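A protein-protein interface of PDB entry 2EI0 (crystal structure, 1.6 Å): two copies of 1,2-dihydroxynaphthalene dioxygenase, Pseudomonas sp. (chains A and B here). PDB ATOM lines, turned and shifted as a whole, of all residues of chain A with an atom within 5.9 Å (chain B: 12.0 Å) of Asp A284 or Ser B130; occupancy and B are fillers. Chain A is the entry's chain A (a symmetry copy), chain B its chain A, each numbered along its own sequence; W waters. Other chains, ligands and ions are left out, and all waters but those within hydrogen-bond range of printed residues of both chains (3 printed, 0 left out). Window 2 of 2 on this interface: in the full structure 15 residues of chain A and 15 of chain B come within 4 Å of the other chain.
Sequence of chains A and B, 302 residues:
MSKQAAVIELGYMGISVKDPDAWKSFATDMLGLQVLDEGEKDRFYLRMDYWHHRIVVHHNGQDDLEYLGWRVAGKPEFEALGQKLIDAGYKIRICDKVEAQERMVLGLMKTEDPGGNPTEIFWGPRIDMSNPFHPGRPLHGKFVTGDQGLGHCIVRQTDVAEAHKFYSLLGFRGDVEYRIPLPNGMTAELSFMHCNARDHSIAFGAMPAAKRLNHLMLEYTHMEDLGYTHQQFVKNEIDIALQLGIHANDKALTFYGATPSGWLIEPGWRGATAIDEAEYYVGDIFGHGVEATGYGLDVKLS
The backbone NH of His B52 is in hydrogen-bond range of the backbone carbonyl oxygen of Arg B126, 3.0 Å away. The side-chain hydroxyl of Tyr A178 sits at hydrogen-bond distance from the backbone NH of Ala A248 (2.9 Å). The backbone carbonyl oxygen of Ile A246 lies within hydrogen-bond range of the backbone NH of Ile A285 (3.0 Å). A ring nitrogen (ND1) of His A247 sits at hydrogen-bond distance from the side-chain carboxylate (OD2) of Asp A284, at 2.8 Å. OD1 of Asp A284 sits at hydrogen-bond distance from N of Ala A248 (2.8 Å). The side-chain carboxylate (OD2) of Asp A284 sits at hydrogen-bond distance from a ring nitrogen (ND1) of His A288, 2.8 Å away.
Among the printed residues, merely in contact across the chains: Asp A284 with Ser B130 (3.4 Å), Val A282 with Arg B126 (3.7 Å), Ile A285 with Met B129 (3.7 Å) and Ala A248 with Met B129 (3.9 Å).
No residue of chain B comes within 4 Å of Gly A245. No residue of chain B comes within 4 Å of His A247. Printed residues of chain B within 4 Å of Val A282: Arg B126. No residue of chain B comes within 4 Å of Gly A283. Of chain B, only Ser B130 comes within 4 Å of Asp A284. Ile A285 touches one residue of chain B. No residue of chain B comes within 4 Å of Gly A287. No residue of chain B comes within 4 Å of His A288. Printed residues of chain A within 4 Å of Arg B126: Val A282. Asp B128 touches none of the printed residues of chain A. Of the printed residues of chain A, Met B129 touches Ala A248 (3.9 Å) and Ile A285 (3.7 Å). Pro B132 touches none of the printed residues of chain A. The nearest residue of chain B that does not touch Asp A284 is Met B129 (5.4 Å). The nearest printed residue of chain A that does not touch Arg B126 is Gly A283 (7.4 Å).
Printed residues of chain B that touch a printed residue of chain A: Arg B126, Met B129 and Ser B130. Of the 13 printed residues of chain A, 4 touch a printed residue of chain B. Hydrophobic or aromatic side chains of chain A within 4 Å of the printed part of chain B: Ala A248, Val A282 and Ile A285. Along chain A the printed residues that touch a printed residue of chain B span positions 248 to 285. Among the printed residues, 4 pairs touch across the chains. Among the printed residues, no Asp or Glu carboxylate lies within 4 Å of a Lys or Arg side-chain nitrogen of the other chain.
No position is printed for both chains. Of the 4 pairs that touch across the chains among the printed residues, none has its exchanged pair printed and touching as well.
Water W2 lies within hydrogen-bond range of the side-chain carboxylate of Asp B128, the backbone NH of Val A282 and the backbone carbonyl oxygen of Ile B127. Water W1 bridges the backbone carbonyl oxygen (O) of Ile A285 (2.9 Å) and the backbone carbonyl oxygen (O) of Ser B130 (2.9 Å). Water W3 lies within hydrogen-bond range of the backbone carbonyl oxygen (O) of Gly A283 (2.9 Å), the backbone NH (N) of Met B129 (3.0 Å) and the backbone NH (N) of Ser B130 (3.1 Å).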
ATOM      1  N   TYR A 178      -7.665 -19.494  -7.637  1.00  0.00           N
ATOM      2  CA  TYR A 178      -7.100 -20.588  -6.860  1.00  0.00           C
ATOM      3  C   TYR A 178      -8.133 -21.199  -5.966  1.00  0.00           C
ATOM      4  O   TYR A 178      -8.919 -20.482  -5.351  1.00  0.00           O
ATOM      5  CB  TYR A 178      -5.942 -20.123  -5.980  1.00  0.00           C
ATOM      6  CG  TYR A 178      -4.677 -19.790  -6.740  1.00  0.00           C
ATOM      7  CD1 TYR A 178      -4.517 -18.541  -7.322  1.00  0.00           C
ATOM      8  CD2 TYR A 178      -3.643 -20.719  -6.870  1.00  0.00           C
ATOM      9  CE1 TYR A 178      -3.359 -18.194  -8.010  1.00  0.00           C
ATOM     10  CE2 TYR A 178      -2.460 -20.376  -7.578  1.00  0.00           C
ATOM     11  CZ  TYR A 178      -2.340 -19.115  -8.126  1.00  0.00           C
ATOM     12  OH  TYR A 178      -1.195 -18.732  -8.816  1.00  0.00           O
ATOM     13  N   GLY A 245       9.279 -18.021  -5.202  1.00  0.00           N
ATOM     14  CA  GLY A 245       8.468 -18.974  -5.941  1.00  0.00           C
ATOM     15  C   GLY A 245       7.835 -18.313  -7.137  1.00  0.00           C
ATOM     16  O   GLY A 245       7.972 -17.098  -7.341  1.00  0.00           O
ATOM     17  N   ILE A 246       7.145 -19.122  -7.935  1.00  0.00           N
ATOM     18  CA  ILE A 246       6.468 -18.606  -9.125  1.00  0.00           C
ATOM     19  C   ILE A 246       4.991 -18.930  -9.056  1.00  0.00           C
ATOM     20  O   ILE A 246       4.602 -20.082  -8.829  1.00  0.00           O
ATOM     21  CB  ILE A 246       7.072 -19.139 -10.424  1.00  0.00           C
ATOM     22  CG1 ILE A 246       8.466 -18.552 -10.640  1.00  0.00           C
ATOM     23  CG2 ILE A 246       6.190 -18.758 -11.627  1.00  0.00           C
ATOM     24  CD1 ILE A 246       9.186 -19.069 -11.883  1.00  0.00           C
ATOM     25  N   HIS A 247       4.186 -17.883  -9.232  1.00  0.00           N
ATOM     26  CA  HIS A 247       2.736 -17.992  -9.215  1.00  0.00           C
ATOM     27  C   HIS A 247       2.218 -18.665 -10.464  1.00  0.00           C
ATOM     28  O   HIS A 247       2.673 -18.352 -11.565  1.00  0.00           O
ATOM     29  CB  HIS A 247       2.117 -16.599  -9.205  1.00  0.00           C
ATOM     30  CG  HIS A 247       2.350 -15.845  -7.946  1.00  0.00           C
ATOM     31  ND1 HIS A 247       2.027 -16.356  -6.703  1.00  0.00           N
ATOM     32  CD2 HIS A 247       2.818 -14.593  -7.732  1.00  0.00           C
ATOM     33  CE1 HIS A 247       2.306 -15.458  -5.778  1.00  0.00           C
ATOM     34  NE2 HIS A 247       2.800 -14.387  -6.375  1.00  0.00           N
ATOM     35  N   ALA A 248       1.221 -19.543 -10.298  1.00  0.00           N
ATOM     36  CA  ALA A 248       0.593 -20.185 -11.457  1.00  0.00           C
ATOM     37  C   ALA A 248      -0.153 -19.181 -12.341  1.00  0.00           C
ATOM     38  O   ALA A 248      -0.156 -19.321 -13.563  1.00  0.00           O
ATOM     39  CB  ALA A 248      -0.327 -21.323 -11.019  1.00  0.00           C
ATOM     40  N   ASN A 249      -0.760 -18.162 -11.731  1.00  0.00           N
ATOM     41  CA  ASN A 249      -1.478 -17.167 -12.529  1.00  0.00           C
ATOM     42  C   ASN A 249      -0.593 -16.167 -13.292  1.00  0.00           C
ATOM     43  O   ASN A 249      -0.629 -16.145 -14.516  1.00  0.00           O
ATOM     44  CB  ASN A 249      -2.642 -16.483 -11.766  1.00  0.00           C
ATOM     45  CG  ASN A 249      -2.211 -15.744 -10.509  1.00  0.00           C
ATOM     46  OD1 ASN A 249      -1.024 -15.610 -10.204  1.00  0.00           O
ATOM     47  ND2 ASN A 249      -3.206 -15.236  -9.774  1.00  0.00           N
ATOM     48  N   VAL A 282      -4.672 -25.191  -8.315  1.00  0.00           N
ATOM     49  CA  VAL A 282      -4.754 -25.651  -6.924  1.00  0.00           C
ATOM     50  C   VAL A 282      -3.407 -25.491  -6.206  1.00  0.00           C
ATOM     51  O   VAL A 282      -3.227 -25.942  -5.077  1.00  0.00           O
ATOM     52  CB  VAL A 282      -5.355 -27.097  -6.807  1.00  0.00           C
ATOM     53  CG1 VAL A 282      -6.741 -27.140  -7.455  1.00  0.00           C
ATOM     54  CG2 VAL A 282      -4.437 -28.155  -7.434  1.00  0.00           C
ATOM     55  N   GLY A 283      -2.477 -24.788  -6.845  1.00  0.00           N
ATOM     56  CA  GLY A 283      -1.180 -24.531  -6.235  1.00  0.00           C
ATOM     57  C   GLY A 283      -0.252 -23.776  -7.163  1.00  0.00           C
ATOM     58  O   GLY A 283      -0.547 -23.605  -8.357  1.00  0.00           O
ATOM     59  N   ASP A 284       0.869 -23.314  -6.613  1.00  0.00           N
ATOM     60  CA  ASP A 284       1.812 -22.544  -7.418  1.00  0.00           C
ATOM     61  C   ASP A 284       2.773 -23.463  -8.199  1.00  0.00           C
ATOM     62  O   ASP A 284       2.731 -24.693  -8.059  1.00  0.00           O
ATOM     63  CB  ASP A 284       2.513 -21.464  -6.569  1.00  0.00           C
ATOM     64  CG  ASP A 284       1.874 -20.066  -6.760  1.00  0.00           C
ATOM     65  OD1 ASP A 284       0.901 -19.933  -7.555  1.00  0.00           O
ATOM     66  OD2 ASP A 284       2.361 -19.078  -6.153  1.00  0.00           O
ATOM     67  N   ILE A 285       3.612 -22.863  -9.043  1.00  0.00           N
ATOM     68  CA  ILE A 285       4.503 -23.639  -9.912  1.00  0.00           C
ATOM     69  C   ILE A 285       5.651 -24.266  -9.105  1.00  0.00           C
ATOM     70  O   ILE A 285       5.947 -25.465  -9.240  1.00  0.00           O
ATOM     71  CB  ILE A 285       4.996 -22.791 -11.101  1.00  0.00           C
ATOM     72  CG1 ILE A 285       3.791 -22.383 -11.962  1.00  0.00           C
ATOM     73  CG2 ILE A 285       6.042 -23.557 -11.921  1.00  0.00           C
ATOM     74  CD1 ILE A 285       4.137 -21.592 -13.231  1.00  0.00           C
ATOM     75  N   PHE A 286       6.278 -23.456  -8.254  1.00  0.00           N
ATOM     76  CA  PHE A 286       7.222 -23.956  -7.266  1.00  0.00           C
ATOM     77  C   PHE A 286       7.364 -22.891  -6.186  1.00  0.00           C
ATOM     78  O   PHE A 286       7.024 -21.721  -6.408  1.00  0.00           O
ATOM     79  CB  PHE A 286       8.595 -24.270  -7.906  1.00  0.00           C
ATOM     80  CG  PHE A 286       9.476 -23.058  -8.102  1.00  0.00           C
ATOM     81  CD1 PHE A 286      10.317 -22.610  -7.078  1.00  0.00           C
ATOM     82  CD2 PHE A 286       9.463 -22.363  -9.309  1.00  0.00           C
ATOM     83  CE1 PHE A 286      11.132 -21.470  -7.254  1.00  0.00           C
ATOM     84  CE2 PHE A 286      10.275 -21.234  -9.490  1.00  0.00           C
ATOM     85  CZ  PHE A 286      11.091 -20.785  -8.469  1.00  0.00           C
ATOM     86  N   GLY A 287       7.885 -23.300  -5.031  1.00  0.00           N
ATOM     87  CA  GLY A 287       8.304 -22.361  -3.989  1.00  0.00           C
ATOM     88  C   GLY A 287       7.140 -21.703  -3.277  1.00  0.00           C
ATOM     89  O   GLY A 287       6.048 -22.277  -3.172  1.00  0.00           O
ATOM     90  N   HIS A 288       7.379 -20.487  -2.793  1.00  0.00           N
ATOM     91  CA  HIS A 288       6.407 -19.765  -1.971  1.00  0.00           C
ATOM     92  C   HIS A 288       6.047 -20.561  -0.719  1.00  0.00           C
ATOM     93  O   HIS A 288       4.899 -20.543  -0.263  1.00  0.00           O
ATOM     94  CB  HIS A 288       5.156 -19.384  -2.765  1.00  0.00           C
ATOM     95  CG  HIS A 288       5.369 -18.246  -3.713  1.00  0.00           C
ATOM     96  ND1 HIS A 288       4.694 -18.139  -4.912  1.00  0.00           N
ATOM     97  CD2 HIS A 288       6.188 -17.168  -3.640  1.00  0.00           C
ATOM     98  CE1 HIS A 288       5.095 -17.047  -5.543  1.00  0.00           C
ATOM     99  NE2 HIS A 288       5.985 -16.428  -4.786  1.00  0.00           N
ATOM    100  N   GLN B  34      -0.609 -38.422 -22.403  1.00  0.00           N
ATOM    101  CA  GLN B  34      -0.204 -38.769 -21.043  1.00  0.00           C
ATOM    102  C   GLN B  34      -1.378 -39.342 -20.264  1.00  0.00           C
ATOM    103  O   GLN B  34      -2.446 -38.731 -20.201  1.00  0.00           O
ATOM    104  CB  GLN B  34       0.343 -37.525 -20.318  1.00  0.00           C
ATOM    105  CG  GLN B  34       0.623 -37.762 -18.814  1.00  0.00           C
ATOM    106  CD  GLN B  34       1.147 -36.522 -18.095  1.00  0.00           C
ATOM    107  OE1 GLN B  34       1.130 -35.408 -18.633  1.00  0.00           O
ATOM    108  NE2 GLN B  34       1.618 -36.715 -16.864  1.00  0.00           N
ATOM    109  N   LEU B  36      -3.165 -39.992 -16.849  1.00  0.00           N
ATOM    110  CA  LEU B  36      -3.246 -39.581 -15.452  1.00  0.00           C
ATOM    111  C   LEU B  36      -4.333 -40.397 -14.751  1.00  0.00           C
ATOM    112  O   LEU B  36      -5.508 -40.327 -15.111  1.00  0.00           O
ATOM    113  CB  LEU B  36      -3.520 -38.071 -15.337  1.00  0.00           C
ATOM    114  CG  LEU B  36      -3.772 -37.484 -13.943  1.00  0.00           C
ATOM    115  CD1 LEU B  36      -2.585 -37.704 -13.012  1.00  0.00           C
ATOM    116  CD2 LEU B  36      -4.122 -35.992 -14.033  1.00  0.00           C
ATOM    117  N   GLU B  38      -6.078 -40.882 -11.256  1.00  0.00           N
ATOM    118  CA  GLU B  38      -6.292 -40.286  -9.934  1.00  0.00           C
ATOM    119  C   GLU B  38      -6.878 -41.299  -8.940  1.00  0.00           C
ATOM    120  O   GLU B  38      -7.358 -40.916  -7.868  1.00  0.00           O
ATOM    121  CB  GLU B  38      -7.213 -39.058 -10.034  1.00  0.00           C
ATOM    122  CG  GLU B  38      -6.669 -37.891 -10.877  1.00  0.00           C
ATOM    123  CD  GLU B  38      -5.799 -36.923 -10.086  1.00  0.00           C
ATOM    124  OE1 GLU B  38      -5.317 -37.281  -8.981  1.00  0.00           O
ATOM    125  OE2 GLU B  38      -5.588 -35.789 -10.563  1.00  0.00           O
ATOM    126  N   ARG B  47      -3.922 -36.407 -20.788  1.00  0.00           N
ATOM    127  CA  ARG B  47      -3.427 -35.036 -20.828  1.00  0.00           C
ATOM    128  C   ARG B  47      -2.706 -34.774 -22.143  1.00  0.00           C
ATOM    129  O   ARG B  47      -2.140 -35.689 -22.750  1.00  0.00           O
ATOM    130  CB  ARG B  47      -2.457 -34.755 -19.685  1.00  0.00           C
ATOM    131  CG  ARG B  47      -2.994 -35.062 -18.285  1.00  0.00           C
ATOM    132  CD  ARG B  47      -1.962 -34.592 -17.276  1.00  0.00           C
ATOM    133  NE  ARG B  47      -1.955 -33.131 -17.062  1.00  0.00           N
ATOM    134  CZ  ARG B  47      -0.855 -32.411 -16.802  1.00  0.00           C
ATOM    135  NH1 ARG B  47       0.354 -32.970 -16.814  1.00  0.00           N
ATOM    136  NH2 ARG B  47      -0.961 -31.119 -16.537  1.00  0.00           N
ATOM    137  N   ASP B  49      -1.200 -31.227 -22.294  1.00  0.00           N
ATOM    138  CA  ASP B  49      -0.632 -29.893 -22.024  1.00  0.00           C
ATOM    139  C   ASP B  49      -0.761 -29.625 -20.532  1.00  0.00           C
ATOM    140  O   ASP B  49      -0.811 -30.569 -19.755  1.00  0.00           O
ATOM    141  CB  ASP B  49      -1.311 -28.795 -22.895  1.00  0.00           C
ATOM    142  CG  ASP B  49      -2.821 -28.711 -22.708  1.00  0.00           C
ATOM    143  OD1 ASP B  49      -3.368 -29.236 -21.704  1.00  0.00           O
ATOM    144  OD2 ASP B  49      -3.472 -28.062 -23.567  1.00  0.00           O
ATOM    145  N   TYR B  50      -0.815 -28.364 -20.114  1.00  0.00           N
ATOM    146  CA  TYR B  50      -0.878 -28.093 -18.668  1.00  0.00           C
ATOM    147  C   TYR B  50      -2.265 -28.328 -18.044  1.00  0.00           C
ATOM    148  O   TYR B  50      -2.397 -28.388 -16.817  1.00  0.00           O
ATOM    149  CB  TYR B  50      -0.471 -26.659 -18.389  1.00  0.00           C
ATOM    150  CG  TYR B  50       1.001 -26.356 -18.380  1.00  0.00           C
ATOM    151  CD1 TYR B  50       1.817 -26.771 -17.328  1.00  0.00           C
ATOM    152  CD2 TYR B  50       1.560 -25.565 -19.385  1.00  0.00           C
ATOM    153  CE1 TYR B  50       3.185 -26.423 -17.287  1.00  0.00           C
ATOM    154  CE2 TYR B  50       2.907 -25.225 -19.371  1.00  0.00           C
ATOM    155  CZ  TYR B  50       3.715 -25.658 -18.319  1.00  0.00           C
ATOM    156  OH  TYR B  50       5.050 -25.308 -18.277  1.00  0.00           O
ATOM    157  N   TRP B  51      -3.310 -28.405 -18.863  1.00  0.00           N
ATOM    158  CA  TRP B  51      -4.638 -28.683 -18.287  1.00  0.00           C
ATOM    159  C   TRP B  51      -4.572 -29.936 -17.435  1.00  0.00           C
ATOM    160  O   TRP B  51      -3.834 -30.875 -17.755  1.00  0.00           O
ATOM    161  CB  TRP B  51      -5.678 -28.850 -19.391  1.00  0.00           C
ATOM    162  CG  TRP B  51      -6.095 -27.539 -20.021  1.00  0.00           C
ATOM    163  CD1 TRP B  51      -5.290 -26.478 -20.368  1.00  0.00           C
ATOM    164  CD2 TRP B  51      -7.425 -27.178 -20.414  1.00  0.00           C
ATOM    165  NE1 TRP B  51      -6.053 -25.475 -20.935  1.00  0.00           N
ATOM    166  CE2 TRP B  51      -7.364 -25.883 -20.972  1.00  0.00           C
ATOM    167  CE3 TRP B  51      -8.668 -27.829 -20.332  1.00  0.00           C
ATOM    168  CZ2 TRP B  51      -8.507 -25.220 -21.448  1.00  0.00           C
ATOM    169  CZ3 TRP B  51      -9.794 -27.187 -20.818  1.00  0.00           C
ATOM    170  CH2 TRP B  51      -9.707 -25.884 -21.366  1.00  0.00           C
ATOM    171  N   HIS B  52      -5.348 -29.976 -16.353  1.00  0.00           N
ATOM    172  CA  HIS B  52      -5.422 -31.207 -15.586  1.00  0.00           C
ATOM    173  C   HIS B  52      -5.693 -32.383 -16.537  1.00  0.00           C
ATOM    174  O   HIS B  52      -5.063 -33.444 -16.437  1.00  0.00           O
ATOM    175  CB  HIS B  52      -6.489 -31.130 -14.497  1.00  0.00           C
ATOM    176  CG  HIS B  52      -6.657 -32.422 -13.767  1.00  0.00           C
ATOM    177  ND1 HIS B  52      -7.492 -33.424 -14.214  1.00  0.00           N
ATOM    178  CD2 HIS B  52      -6.049 -32.902 -12.655  1.00  0.00           C
ATOM    179  CE1 HIS B  52      -7.406 -34.460 -13.396  1.00  0.00           C
ATOM    180  NE2 HIS B  52      -6.536 -34.170 -12.446  1.00  0.00           N
ATOM    181  N   HIS B  53      -6.617 -32.173 -17.478  1.00  0.00           N
ATOM    182  CA  HIS B  53      -6.847 -33.172 -18.523  1.00  0.00           C
ATOM    183  C   HIS B  53      -7.540 -32.542 -19.711  1.00  0.00           C
ATOM    184  O   HIS B  53      -8.153 -31.466 -19.589  1.00  0.00           O
ATOM    185  CB  HIS B  53      -7.707 -34.301 -17.983  1.00  0.00           C
ATOM    186  CG  HIS B  53      -9.082 -33.872 -17.565  1.00  0.00           C
ATOM    187  ND1 HIS B  53      -9.388 -33.535 -16.263  1.00  0.00           N
ATOM    188  CD2 HIS B  53     -10.230 -33.731 -18.269  1.00  0.00           C
ATOM    189  CE1 HIS B  53     -10.664 -33.201 -16.184  1.00  0.00           C
ATOM    190  NE2 HIS B  53     -11.197 -33.307 -17.388  1.00  0.00           N
ATOM    191  N   PRO B 125     -11.527 -23.799 -16.531  1.00  0.00           N
ATOM    192  CA  PRO B 125     -10.907 -25.116 -16.423  1.00  0.00           C
ATOM    193  C   PRO B 125      -9.805 -25.107 -15.365  1.00  0.00           C
ATOM    194  O   PRO B 125      -9.244 -24.045 -15.057  1.00  0.00           O
ATOM    195  CB  PRO B 125     -10.262 -25.298 -17.800  1.00  0.00           C
ATOM    196  CG  PRO B 125      -9.933 -23.894 -18.234  1.00  0.00           C
ATOM    197  CD  PRO B 125     -11.143 -23.112 -17.783  1.00  0.00           C
ATOM    198  N   ARG B 126      -9.517 -26.287 -14.828  1.00  0.00           N
ATOM    199  CA  ARG B 126      -8.401 -26.484 -13.914  1.00  0.00           C
ATOM    200  C   ARG B 126      -7.124 -26.693 -14.704  1.00  0.00           C
ATOM    201  O   ARG B 126      -7.026 -27.608 -15.537  1.00  0.00           O
ATOM    202  CB  ARG B 126      -8.639 -27.701 -13.016  1.00  0.00           C
ATOM    203  CG  ARG B 126      -7.441 -27.981 -12.105  1.00  0.00           C
ATOM    204  CD  ARG B 126      -7.671 -29.178 -11.206  1.00  0.00           C
ATOM    205  NE  ARG B 126      -6.405 -29.756 -10.746  1.00  0.00           N
ATOM    206  CZ  ARG B 126      -6.312 -30.696  -9.807  1.00  0.00           C
ATOM    207  NH1 ARG B 126      -7.411 -31.138  -9.207  1.00  0.00           N
ATOM    208  NH2 ARG B 126      -5.131 -31.181  -9.458  1.00  0.00           N
ATOM    209  N   ILE B 127      -6.146 -25.839 -14.437  1.00  0.00           N
ATOM    210  CA  ILE B 127      -4.844 -25.911 -15.083  1.00  0.00           C
ATOM    211  C   ILE B 127      -3.803 -26.310 -14.047  1.00  0.00           C
ATOM    212  O   ILE B 127      -3.686 -25.668 -12.990  1.00  0.00           O
ATOM    213  CB  ILE B 127      -4.435 -24.548 -15.677  1.00  0.00           C
ATOM    214  CG1 ILE B 127      -5.573 -23.923 -16.496  1.00  0.00           C
ATOM    215  CG2 ILE B 127      -3.111 -24.661 -16.481  1.00  0.00           C
ATOM    216  CD1 ILE B 127      -6.187 -24.811 -17.528  1.00  0.00           C
ATOM    217  N   ASP B 128      -3.065 -27.381 -14.314  1.00  0.00           N
ATOM    218  CA  ASP B 128      -2.022 -27.773 -13.379  1.00  0.00           C
ATOM    219  C   ASP B 128      -0.656 -27.288 -13.844  1.00  0.00           C
ATOM    220  O   ASP B 128       0.172 -28.044 -14.362  1.00  0.00           O
ATOM    221  CB  ASP B 128      -2.059 -29.276 -13.136  1.00  0.00           C
ATOM    222  CG  ASP B 128      -3.279 -29.701 -12.341  1.00  0.00           C
ATOM    223  OD1 ASP B 128      -3.913 -28.847 -11.663  1.00  0.00           O
ATOM    224  OD2 ASP B 128      -3.595 -30.893 -12.410  1.00  0.00           O
ATOM    225  N   MET B 129      -0.421 -26.001 -13.626  1.00  0.00           N
ATOM    226  CA  MET B 129       0.866 -25.385 -13.974  1.00  0.00           C
ATOM    227  C   MET B 129       2.063 -26.025 -13.264  1.00  0.00           C
ATOM    228  O   MET B 129       3.182 -25.971 -13.768  1.00  0.00           O
ATOM    229  CB  MET B 129       0.837 -23.878 -13.685  1.00  0.00           C
ATOM    230  CG  MET B 129      -0.069 -23.076 -14.611  1.00  0.00           C
ATOM    231  SD  MET B 129       0.236 -23.336 -16.385  1.00  0.00           S
ATOM    232  CE  MET B 129       1.964 -22.935 -16.531  1.00  0.00           C
ATOM    233  N   SER B 130       1.828 -26.594 -12.079  1.00  0.00           N
ATOM    234  CA  SER B 130       2.883 -27.271 -11.313  1.00  0.00           C
ATOM    235  C   SER B 130       3.289 -28.613 -11.938  1.00  0.00           C
ATOM    236  O   SER B 130       4.316 -29.189 -11.552  1.00  0.00           O
ATOM    237  CB  SER B 130       2.398 -27.533  -9.884  1.00  0.00           C
ATOM    238  OG  SER B 130       1.284 -28.401  -9.915  1.00  0.00           O
ATOM    239  N   ASN B 131       2.473 -29.111 -12.870  1.00  0.00           N
ATOM    240  CA  ASN B 131       2.630 -30.452 -13.410  1.00  0.00           C
ATOM    241  C   ASN B 131       2.733 -30.415 -14.927  1.00  0.00           C
ATOM    242  O   ASN B 131       1.750 -30.639 -15.634  1.00  0.00           O
ATOM    243  CB  ASN B 131       1.442 -31.332 -12.987  1.00  0.00           C
ATOM    244  CG  ASN B 131       1.661 -32.809 -13.294  1.00  0.00           C
ATOM    245  OD1 ASN B 131       2.802 -33.280 -13.448  1.00  0.00           O
ATOM    246  ND2 ASN B 131       0.560 -33.551 -13.394  1.00  0.00           N
ATOM    247  N   PRO B 132       3.930 -30.118 -15.442  1.00  0.00           N
ATOM    248  CA  PRO B 132       4.042 -30.009 -16.900  1.00  0.00           C
ATOM    249  C   PRO B 132       3.707 -31.311 -17.628  1.00  0.00           C
ATOM    250  O   PRO B 132       3.908 -32.417 -17.093  1.00  0.00           O
ATOM    251  CB  PRO B 132       5.513 -29.606 -17.125  1.00  0.00           C
ATOM    252  CG  PRO B 132       6.213 -29.881 -15.861  1.00  0.00           C
ATOM    253  CD  PRO B 132       5.209 -29.865 -14.753  1.00  0.00           C
ATOM    254  N   PHE B 133       3.177 -31.160 -18.840  1.00  0.00           N
ATOM    255  CA  PHE B 133       2.884 -32.308 -19.690  1.00  0.00           C
ATOM    256  C   PHE B 133       4.101 -33.227 -19.798  1.00  0.00           C
ATOM    257  O   PHE B 133       5.238 -32.764 -19.975  1.00  0.00           O
ATOM    258  CB  PHE B 133       2.419 -31.824 -21.075  1.00  0.00           C
ATOM    259  CG  PHE B 133       2.247 -32.926 -22.088  1.00  0.00           C
ATOM    260  CD1 PHE B 133       1.258 -33.901 -21.933  1.00  0.00           C
ATOM    261  CD2 PHE B 133       3.071 -32.981 -23.217  1.00  0.00           C
ATOM    262  CE1 PHE B 133       1.093 -34.925 -22.881  1.00  0.00           C
ATOM    263  CE2 PHE B 133       2.905 -33.994 -24.172  1.00  0.00           C
ATOM    264  CZ  PHE B 133       1.919 -34.970 -23.995  1.00  0.00           C
ATOM    265  N   HIS B 134       3.847 -34.525 -19.683  1.00  0.00           N
ATOM    266  CA  HIS B 134       4.897 -35.521 -19.827  1.00  0.00           C
ATOM    267  C   HIS B 134       4.320 -36.618 -20.699  1.00  0.00           C
ATOM    268  O   HIS B 134       3.476 -37.398 -20.249  1.00  0.00           O
ATOM    269  CB  HIS B 134       5.323 -36.054 -18.460  1.00  0.00           C
ATOM    270  CG  HIS B 134       6.589 -36.847 -18.489  1.00  0.00           C
ATOM    271  ND1 HIS B 134       7.769 -36.355 -19.009  1.00  0.00           N
ATOM    272  CD2 HIS B 134       6.867 -38.094 -18.038  1.00  0.00           C
ATOM    273  CE1 HIS B 134       8.712 -37.276 -18.897  1.00  0.00           C
ATOM    274  NE2 HIS B 134       8.192 -38.337 -18.303  1.00  0.00           N
HETATM  275  O   HOH W   1       6.491 -27.211 -11.430  1.00  0.00           O
HETATM  276  O   HOH W   2      -3.006 -26.604 -10.182  1.00  0.00           O
HETATM  277  O   HOH W   3      -0.650 -25.222 -10.712  1.00  0.00           O
